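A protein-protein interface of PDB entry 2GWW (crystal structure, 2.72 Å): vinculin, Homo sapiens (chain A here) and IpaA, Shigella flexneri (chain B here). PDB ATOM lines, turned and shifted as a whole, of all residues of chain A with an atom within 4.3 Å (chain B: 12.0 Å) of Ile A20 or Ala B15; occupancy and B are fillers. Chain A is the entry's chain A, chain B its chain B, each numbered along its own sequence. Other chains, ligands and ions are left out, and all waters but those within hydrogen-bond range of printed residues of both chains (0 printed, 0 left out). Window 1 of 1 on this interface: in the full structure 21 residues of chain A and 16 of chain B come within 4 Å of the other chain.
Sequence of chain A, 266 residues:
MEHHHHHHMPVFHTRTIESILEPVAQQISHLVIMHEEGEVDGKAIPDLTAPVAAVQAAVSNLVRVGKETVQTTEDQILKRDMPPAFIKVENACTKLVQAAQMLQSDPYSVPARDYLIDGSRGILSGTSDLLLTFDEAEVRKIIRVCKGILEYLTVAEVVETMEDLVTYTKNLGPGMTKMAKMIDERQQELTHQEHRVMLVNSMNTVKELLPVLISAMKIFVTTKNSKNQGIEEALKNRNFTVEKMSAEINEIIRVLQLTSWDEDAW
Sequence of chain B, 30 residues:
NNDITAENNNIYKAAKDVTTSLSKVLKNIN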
ATOM      1  N   THR A  16      14.034   7.567  -8.993  1.00  0.00           N
ATOM      2  CA  THR A  16      13.348   8.808  -8.644  1.00  0.00           C
ATOM      3  C   THR A  16      13.390   9.039  -7.140  1.00  0.00           C
ATOM      4  O   THR A  16      14.036   9.967  -6.660  1.00  0.00           O
ATOM      5  CB  THR A  16      11.888   8.798  -9.130  1.00  0.00           C
ATOM      6  OG1 THR A  16      11.857   8.723 -10.560  1.00  0.00           O
ATOM      7  CG2 THR A  16      11.161  10.058  -8.671  1.00  0.00           C
ATOM      8  N   ILE A  17      12.684   8.187  -6.404  1.00  0.00           N
ATOM      9  CA  ILE A  17      12.623   8.273  -4.948  1.00  0.00           C
ATOM     10  C   ILE A  17      14.007   8.436  -4.328  1.00  0.00           C
ATOM     11  O   ILE A  17      14.235   9.344  -3.529  1.00  0.00           O
ATOM     12  CB  ILE A  17      11.931   7.030  -4.360  1.00  0.00           C
ATOM     13  CG1 ILE A  17      10.537   6.853  -4.968  1.00  0.00           C
ATOM     14  CG2 ILE A  17      11.865   7.134  -2.837  1.00  0.00           C
ATOM     15  CD1 ILE A  17       9.832   5.576  -4.535  1.00  0.00           C
ATOM     16  N   GLU A  18      14.920   7.541  -4.694  1.00  0.00           N
ATOM     17  CA  GLU A  18      16.282   7.560  -4.162  1.00  0.00           C
ATOM     18  C   GLU A  18      16.979   8.904  -4.369  1.00  0.00           C
ATOM     19  O   GLU A  18      17.608   9.432  -3.452  1.00  0.00           O
ATOM     20  CB  GLU A  18      17.110   6.428  -4.767  1.00  0.00           C
ATOM     21  CG  GLU A  18      18.483   6.854  -5.237  1.00  0.00           C
ATOM     22  CD  GLU A  18      19.364   5.672  -5.581  1.00  0.00           C
ATOM     23  OE1 GLU A  18      19.474   4.749  -4.744  1.00  0.00           O
ATOM     24  OE2 GLU A  18      19.929   5.659  -6.697  1.00  0.00           O
ATOM     25  N   SER A  19      16.861   9.458  -5.568  1.00  0.00           N
ATOM     26  CA  SER A  19      17.468  10.748  -5.866  1.00  0.00           C
ATOM     27  C   SER A  19      16.892  11.830  -4.950  1.00  0.00           C
ATOM     28  O   SER A  19      17.487  12.895  -4.775  1.00  0.00           O
ATOM     29  CB  SER A  19      17.233  11.120  -7.328  1.00  0.00           C
ATOM     30  OG  SER A  19      16.088  11.937  -7.460  1.00  0.00           O
ATOM     31  N   ILE A  20      15.735  11.540  -4.362  1.00  0.00           N
ATOM     32  CA  ILE A  20      15.054  12.473  -3.466  1.00  0.00           C
ATOM     33  C   ILE A  20      15.431  12.250  -2.010  1.00  0.00           C
ATOM     34  O   ILE A  20      15.676  13.199  -1.269  1.00  0.00           O
ATOM     35  CB  ILE A  20      13.525  12.358  -3.609  1.00  0.00           C
ATOM     36  CG1 ILE A  20      13.080  12.725  -5.022  1.00  0.00           C
ATOM     37  CG2 ILE A  20      12.815  13.226  -2.578  1.00  0.00           C
ATOM     38  CD1 ILE A  20      11.615  13.110  -5.111  1.00  0.00           C
ATOM     39  N   LEU A  21      15.451  10.987  -1.600  1.00  0.00           N
ATOM     40  CA  LEU A  21      15.746  10.638  -0.217  1.00  0.00           C
ATOM     41  C   LEU A  21      17.225  10.405   0.081  1.00  0.00           C
ATOM     42  O   LEU A  21      17.678  10.642   1.197  1.00  0.00           O
ATOM     43  CB  LEU A  21      14.917   9.426   0.206  1.00  0.00           C
ATOM     44  CG  LEU A  21      13.412   9.588  -0.009  1.00  0.00           C
ATOM     45  CD1 LEU A  21      12.633   8.648   0.888  1.00  0.00           C
ATOM     46  CD2 LEU A  21      13.000  11.028   0.242  1.00  0.00           C
ATOM     47  N   GLU A  22      17.969   9.938  -0.916  1.00  0.00           N
ATOM     48  CA  GLU A  22      19.394   9.651  -0.751  1.00  0.00           C
ATOM     49  C   GLU A  22      20.211  10.771  -0.117  1.00  0.00           C
ATOM     50  O   GLU A  22      20.995  10.542   0.807  1.00  0.00           O
ATOM     51  CB  GLU A  22      20.020   9.228  -2.081  1.00  0.00           C
ATOM     52  CG  GLU A  22      21.406   8.614  -1.952  1.00  0.00           C
ATOM     53  CD  GLU A  22      21.389   7.284  -1.227  1.00  0.00           C
ATOM     54  OE1 GLU A  22      20.612   7.144  -0.257  1.00  0.00           O
ATOM     55  OE2 GLU A  22      22.158   6.382  -1.619  1.00  0.00           O
ATOM     56  N   PRO A  23      20.047  12.002  -0.616  1.00  0.00           N
ATOM     57  CA  PRO A  23      20.796  13.149  -0.098  1.00  0.00           C
ATOM     58  C   PRO A  23      20.654  13.313   1.414  1.00  0.00           C
ATOM     59  O   PRO A  23      21.620  13.137   2.158  1.00  0.00           O
ATOM     60  CB  PRO A  23      20.161  14.339  -0.825  1.00  0.00           C
ATOM     61  CG  PRO A  23      19.550  13.759  -2.051  1.00  0.00           C
ATOM     62  CD  PRO A  23      19.086  12.390  -1.661  1.00  0.00           C
ATOM     63  N   VAL A  24      19.450  13.661   1.865  1.00  0.00           N
ATOM     64  CA  VAL A  24      19.185  13.856   3.290  1.00  0.00           C
ATOM     65  C   VAL A  24      19.333  12.559   4.077  1.00  0.00           C
ATOM     66  O   VAL A  24      19.619  12.584   5.273  1.00  0.00           O
ATOM     67  CB  VAL A  24      17.787  14.466   3.535  1.00  0.00           C
ATOM     68  CG1 VAL A  24      17.774  15.952   3.224  1.00  0.00           C
ATOM     69  CG2 VAL A  24      16.731  13.729   2.724  1.00  0.00           C
ATOM     70  N   LEU A 131       5.958   8.186  -0.782  1.00  0.00           N
ATOM     71  CA  LEU A 131       6.433   7.845  -2.117  1.00  0.00           C
ATOM     72  C   LEU A 131       6.229   6.358  -2.393  1.00  0.00           C
ATOM     73  O   LEU A 131       5.774   5.977  -3.469  1.00  0.00           O
ATOM     74  CB  LEU A 131       7.912   8.207  -2.277  1.00  0.00           C
ATOM     75  CG  LEU A 131       8.298   9.688  -2.211  1.00  0.00           C
ATOM     76  CD1 LEU A 131       9.817   9.836  -2.147  1.00  0.00           C
ATOM     77  CD2 LEU A 131       7.733  10.457  -3.393  1.00  0.00           C
ATOM     78  N   ASN B   9       5.254  12.519 -10.477  1.00  0.00           N
ATOM     79  CA  ASN B   9       4.747  13.748 -11.075  1.00  0.00           C
ATOM     80  C   ASN B   9       4.837  14.926 -10.103  1.00  0.00           C
ATOM     81  O   ASN B   9       5.929  15.376  -9.746  1.00  0.00           O
ATOM     82  CB  ASN B   9       3.300  13.553 -11.528  1.00  0.00           C
ATOM     83  CG  ASN B   9       2.426  12.967 -10.438  1.00  0.00           C
ATOM     84  OD1 ASN B   9       2.840  12.062  -9.714  1.00  0.00           O
ATOM     85  ND2 ASN B   9       1.210  13.488 -10.310  1.00  0.00           N
ATOM     86  N   ASN B  10       3.677  15.427  -9.686  1.00  0.00           N
ATOM     87  CA  ASN B  10       3.603  16.553  -8.766  1.00  0.00           C
ATOM     88  C   ASN B  10       3.939  16.108  -7.348  1.00  0.00           C
ATOM     89  O   ASN B  10       4.288  16.922  -6.493  1.00  0.00           O
ATOM     90  CB  ASN B  10       2.209  17.178  -8.800  1.00  0.00           C
ATOM     91  CG  ASN B  10       2.196  18.598  -8.281  1.00  0.00           C
ATOM     92  OD1 ASN B  10       2.708  18.879  -7.196  1.00  0.00           O
ATOM     93  ND2 ASN B  10       1.628  19.510  -9.061  1.00  0.00           N
ATOM     94  N   ILE B  11       3.833  14.803  -7.109  1.00  0.00           N
ATOM     95  CA  ILE B  11       4.128  14.226  -5.799  1.00  0.00           C
ATOM     96  C   ILE B  11       5.635  14.197  -5.563  1.00  0.00           C
ATOM     97  O   ILE B  11       6.104  14.419  -4.448  1.00  0.00           O
ATOM     98  CB  ILE B  11       3.543  12.801  -5.664  1.00  0.00           C
ATOM     99  CG1 ILE B  11       2.018  12.832  -5.745  1.00  0.00           C
ATOM    100  CG2 ILE B  11       3.993  12.162  -4.357  1.00  0.00           C
ATOM    101  CD1 ILE B  11       1.478  12.871  -7.169  1.00  0.00           C
ATOM    102  N   TYR B  12       6.385  13.907  -6.621  1.00  0.00           N
ATOM    103  CA  TYR B  12       7.838  13.848  -6.532  1.00  0.00           C
ATOM    104  C   TYR B  12       8.423  15.249  -6.425  1.00  0.00           C
ATOM    105  O   TYR B  12       9.494  15.441  -5.855  1.00  0.00           O
ATOM    106  CB  TYR B  12       8.424  13.125  -7.745  1.00  0.00           C
ATOM    107  CG  TYR B  12       7.821  11.763  -7.995  1.00  0.00           C
ATOM    108  CD1 TYR B  12       7.486  11.355  -9.279  1.00  0.00           C
ATOM    109  CD2 TYR B  12       7.588  10.881  -6.947  1.00  0.00           C
ATOM    110  CE1 TYR B  12       6.928  10.114  -9.513  1.00  0.00           C
ATOM    111  CE2 TYR B  12       7.037   9.633  -7.175  1.00  0.00           C
ATOM    112  CZ  TYR B  12       6.706   9.256  -8.459  1.00  0.00           C
ATOM    113  OH  TYR B  12       6.158   8.016  -8.693  1.00  0.00           O
ATOM    114  N   LYS B  13       7.712  16.229  -6.976  1.00  0.00           N
ATOM    115  CA  LYS B  13       8.163  17.611  -6.927  1.00  0.00           C
ATOM    116  C   LYS B  13       8.168  18.112  -5.488  1.00  0.00           C
ATOM    117  O   LYS B  13       9.194  18.577  -4.986  1.00  0.00           O
ATOM    118  CB  LYS B  13       7.277  18.505  -7.800  1.00  0.00           C
ATOM    119  CG  LYS B  13       8.027  19.645  -8.481  1.00  0.00           C
ATOM    120  CD  LYS B  13       7.073  20.652  -9.111  1.00  0.00           C
ATOM    121  CE  LYS B  13       7.547  22.082  -8.882  1.00  0.00           C
ATOM    122  NZ  LYS B  13       7.835  22.787 -10.168  1.00  0.00           N
ATOM    123  N   ALA B  14       7.022  17.995  -4.823  1.00  0.00           N
ATOM    124  CA  ALA B  14       6.895  18.423  -3.434  1.00  0.00           C
ATOM    125  C   ALA B  14       7.884  17.694  -2.522  1.00  0.00           C
ATOM    126  O   ALA B  14       8.460  18.291  -1.608  1.00  0.00           O
ATOM    127  CB  ALA B  14       5.481  18.207  -2.953  1.00  0.00           C
ATOM    128  N   ALA B  15       8.059  16.397  -2.762  1.00  0.00           N
ATOM    129  CA  ALA B  15       8.968  15.582  -1.965  1.00  0.00           C
ATOM    130  C   ALA B  15      10.389  16.139  -1.980  1.00  0.00           C
ATOM    131  O   ALA B  15      11.048  16.205  -0.940  1.00  0.00           O
ATOM    132  CB  ALA B  15       8.953  14.147  -2.456  1.00  0.00           C
ATOM    133  N   LYS B  16      10.856  16.532  -3.162  1.00  0.00           N
ATOM    134  CA  LYS B  16      12.196  17.085  -3.310  1.00  0.00           C
ATOM    135  C   LYS B  16      12.302  18.391  -2.532  1.00  0.00           C
ATOM    136  O   LYS B  16      13.302  18.653  -1.866  1.00  0.00           O
ATOM    137  CB  LYS B  16      12.513  17.322  -4.788  1.00  0.00           C
ATOM    138  CG  LYS B  16      13.978  17.618  -5.076  1.00  0.00           C
ATOM    139  CD  LYS B  16      14.138  18.410  -6.367  1.00  0.00           C
ATOM    140  CE  LYS B  16      13.189  19.597  -6.411  1.00  0.00           C
ATOM    141  NZ  LYS B  16      13.652  20.647  -7.363  1.00  0.00           N
ATOM    142  N   ASP B  17      11.251  19.200  -2.608  1.00  0.00           N
ATOM    143  CA  ASP B  17      11.226  20.474  -1.903  1.00  0.00           C
ATOM    144  C   ASP B  17      11.498  20.235  -0.427  1.00  0.00           C
ATOM    145  O   ASP B  17      12.319  20.912   0.190  1.00  0.00           O
ATOM    146  CB  ASP B  17       9.867  21.152  -2.082  1.00  0.00           C
ATOM    147  CG  ASP B  17       9.606  21.567  -3.518  1.00  0.00           C
ATOM    148  OD1 ASP B  17       8.422  21.724  -3.886  1.00  0.00           O
ATOM    149  OD2 ASP B  17      10.586  21.746  -4.277  1.00  0.00           O
ATOM    150  N   VAL B  18      10.807  19.245   0.126  1.00  0.00           N
ATOM    151  CA  VAL B  18      10.968  18.866   1.526  1.00  0.00           C
ATOM    152  C   VAL B  18      12.425  18.527   1.821  1.00  0.00           C
ATOM    153  O   VAL B  18      13.043  19.111   2.708  1.00  0.00           O
ATOM    154  CB  VAL B  18      10.075  17.663   1.859  1.00  0.00           C
ATOM    155  CG1 VAL B  18      10.609  16.912   3.071  1.00  0.00           C
ATOM    156  CG2 VAL B  18       8.642  18.109   2.083  1.00  0.00           C
ATOM    157  N   THR B  19      12.965  17.577   1.062  1.00  0.00           N
ATOM    158  CA  THR B  19      14.347  17.140   1.233  1.00  0.00           C
ATOM    159  C   THR B  19      15.367  18.239   0.947  1.00  0.00           C
ATOM    160  O   THR B  19      16.438  18.275   1.556  1.00  0.00           O
ATOM    161  CB  THR B  19      14.649  15.894   0.387  1.00  0.00           C
ATOM    162  OG1 THR B  19      14.128  16.080  -0.939  1.00  0.00           O
ATOM    163  CG2 THR B  19      14.023  14.658   1.007  1.00  0.00           C
ATOM    164  N   THR B  20      15.048  19.125   0.004  1.00  0.00           N
ATOM    165  CA  THR B  20      15.954  20.221  -0.356  1.00  0.00           C
ATOM    166  C   THR B  20      16.086  21.209   0.793  1.00  0.00           C
ATOM    167  O   THR B  20      17.190  21.519   1.239  1.00  0.00           O
ATOM    168  CB  THR B  20      15.487  20.980  -1.616  1.00  0.00           C
ATOM    169  OG1 THR B  20      14.942  20.068  -2.573  1.00  0.00           O
ATOM    170  CG2 THR B  20      16.652  21.731  -2.244  1.00  0.00           C
ATOM    171  N   SER B  21      14.947  21.716   1.256  1.00  0.00           N
ATOM    172  CA  SER B  21      14.921  22.681   2.351  1.00  0.00           C
ATOM    173  C   SER B  21      15.453  22.086   3.655  1.00  0.00           C
ATOM    174  O   SER B  21      15.993  22.802   4.501  1.00  0.00           O
ATOM    175  CB  SER B  21      13.509  23.243   2.548  1.00  0.00           C
ATOM    176  OG  SER B  21      12.558  22.208   2.729  1.00  0.00           O
ATOM    177  N   LEU B  22      15.303  20.773   3.809  1.00  0.00           N
ATOM    178  CA  LEU B  22      15.776  20.077   4.999  1.00  0.00           C
ATOM    179  C   LEU B  22      17.269  19.776   4.910  1.00  0.00           C
ATOM    180  O   LEU B  22      17.924  19.538   5.924  1.00  0.00           O
ATOM    181  CB  LEU B  22      14.991  18.782   5.220  1.00  0.00           C
ATOM    182  CG  LEU B  22      15.446  17.898   6.386  1.00  0.00           C
ATOM    183  CD1 LEU B  22      14.497  18.028   7.568  1.00  0.00           C
ATOM    184  CD2 LEU B  22      15.575  16.442   5.957  1.00  0.00           C
ATOM    185  N   SER B  23      17.803  19.791   3.694  1.00  0.00           N
ATOM    186  CA  SER B  23      19.226  19.548   3.483  1.00  0.00           C
ATOM    187  C   SER B  23      20.011  20.779   3.922  1.00  0.00           C
ATOM    188  O   SER B  23      21.011  20.672   4.632  1.00  0.00           O
ATOM    189  CB  SER B  23      19.506  19.247   2.008  1.00  0.00           C
ATOM    190  OG  SER B  23      19.693  17.859   1.792  1.00  0.00           O
ATOM    191  N   LYS B  24      19.536  21.952   3.512  1.00  0.00           N
ATOM    192  CA  LYS B  24      20.184  23.208   3.866  1.00  0.00           C
ATOM    193  C   LYS B  24      20.043  23.507   5.356  1.00  0.00           C
ATOM    194  O   LYS B  24      20.610  24.474   5.858  1.00  0.00           O
ATOM    195  CB  LYS B  24      19.624  24.361   3.031  1.00  0.00           C
ATOM    196  CG  LYS B  24      20.315  24.543   1.686  1.00  0.00           C
ATOM    197  CD  LYS B  24      20.379  23.232   0.917  1.00  0.00           C
ATOM    198  CE  LYS B  24      20.232  23.457  -0.582  1.00  0.00           C
ATOM    199  NZ  LYS B  24      20.091  24.901  -0.916  1.00  0.00           N
ATOM    200  N   LEU B  26      20.263  20.741   7.859  1.00  0.00           N
ATOM    201  CA  LEU B  26      21.188  19.833   8.522  1.00  0.00           C
ATOM    202  C   LEU B  26      22.628  20.176   8.164  1.00  0.00           C
ATOM    203  O   LEU B  26      23.545  19.940   8.949  1.00  0.00           O
ATOM    204  CB  LEU B  26      20.881  18.386   8.136  1.00  0.00           C
ATOM    205  CG  LEU B  26      19.411  17.968   8.208  1.00  0.00           C
ATOM    206  CD1 LEU B  26      19.211  16.579   7.627  1.00  0.00           C
ATOM    207  CD2 LEU B  26      18.906  18.032   9.640  1.00  0.00           C
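Tyr B12 touches Thr A16. Ile A20 touches Tyr B12. Ile A20 touches Ala B15. CG2 of Ile A20 touches N of Lys B16, 3.9 Å away. CD2 of Leu A21 touches CG2 of Thr B19, at 3.8 Å. Val A24 touches Thr B19. CG1 of Val A24 touches CD2 of Leu B22 (3.5 Å). CG1 of Val A24 touches OG of Ser B23 (3.1 Å). Tyr B12 touches Leu A131 (CD2 to CD2, 3.6 Å). Leu A131 touches Ala B15 (CD2 to CB, 3.998 Å).
Of chain B, only Tyr B12 (3.8 Å) comes within 4 Å of Thr A16. Ile A17 touches none of the printed residues of chain B. No residue of chain B comes within 4 Å of Glu A18. Of chain B, only Tyr B12 (3.2 Å), Ala B15 (3.8 Å), Lys B16 (3.9 Å) and Thr B19 (3.2 Å) come within 4 Å of Ile A20. Of chain B, only Thr B19, Leu B22 and Ser B23 come within 4 Å of Val A24. Of the printed residues of chain B, Leu A131 touches Tyr B12 (3.6 Å) and Ala B15 (3.998 Å). Of the printed residues of chain A, Ala B15 touches Ile A20 (3.8 Å) and Leu A131 (3.998 Å). Val B18 touches none of the printed residues of chain A. Of the printed residues of chain A, Ser B23 touches Val A24. The nearest residue of chain B that does not touch Ile A20 is Lys B13 (5.3 Å).
Hydrophobic or aromatic side chains of chain B within 4 Å of the printed part of chain A: Tyr B12, Ala B15 and Leu B22. Along chain B the printed residues that touch a printed residue of chain A span positions 12 to 23.
The backbone carbonyl oxygen of Ile A20 sits close to the side-chain hydroxyl of Thr B19 (3.3 Å).
O of Thr A16 is in hydrogen-bond range of OG of Ser A19. O of Ala B15 is in hydrogen-bond range of OG1 of Thr B19 (3.1 Å). The side-chain hydroxyl of Thr B19 is in hydrogen-bond range of the backbone carbonyl oxygen of Lys B16. OG of Ser B23 sits close to O of Thr B19 (3.3 Å).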
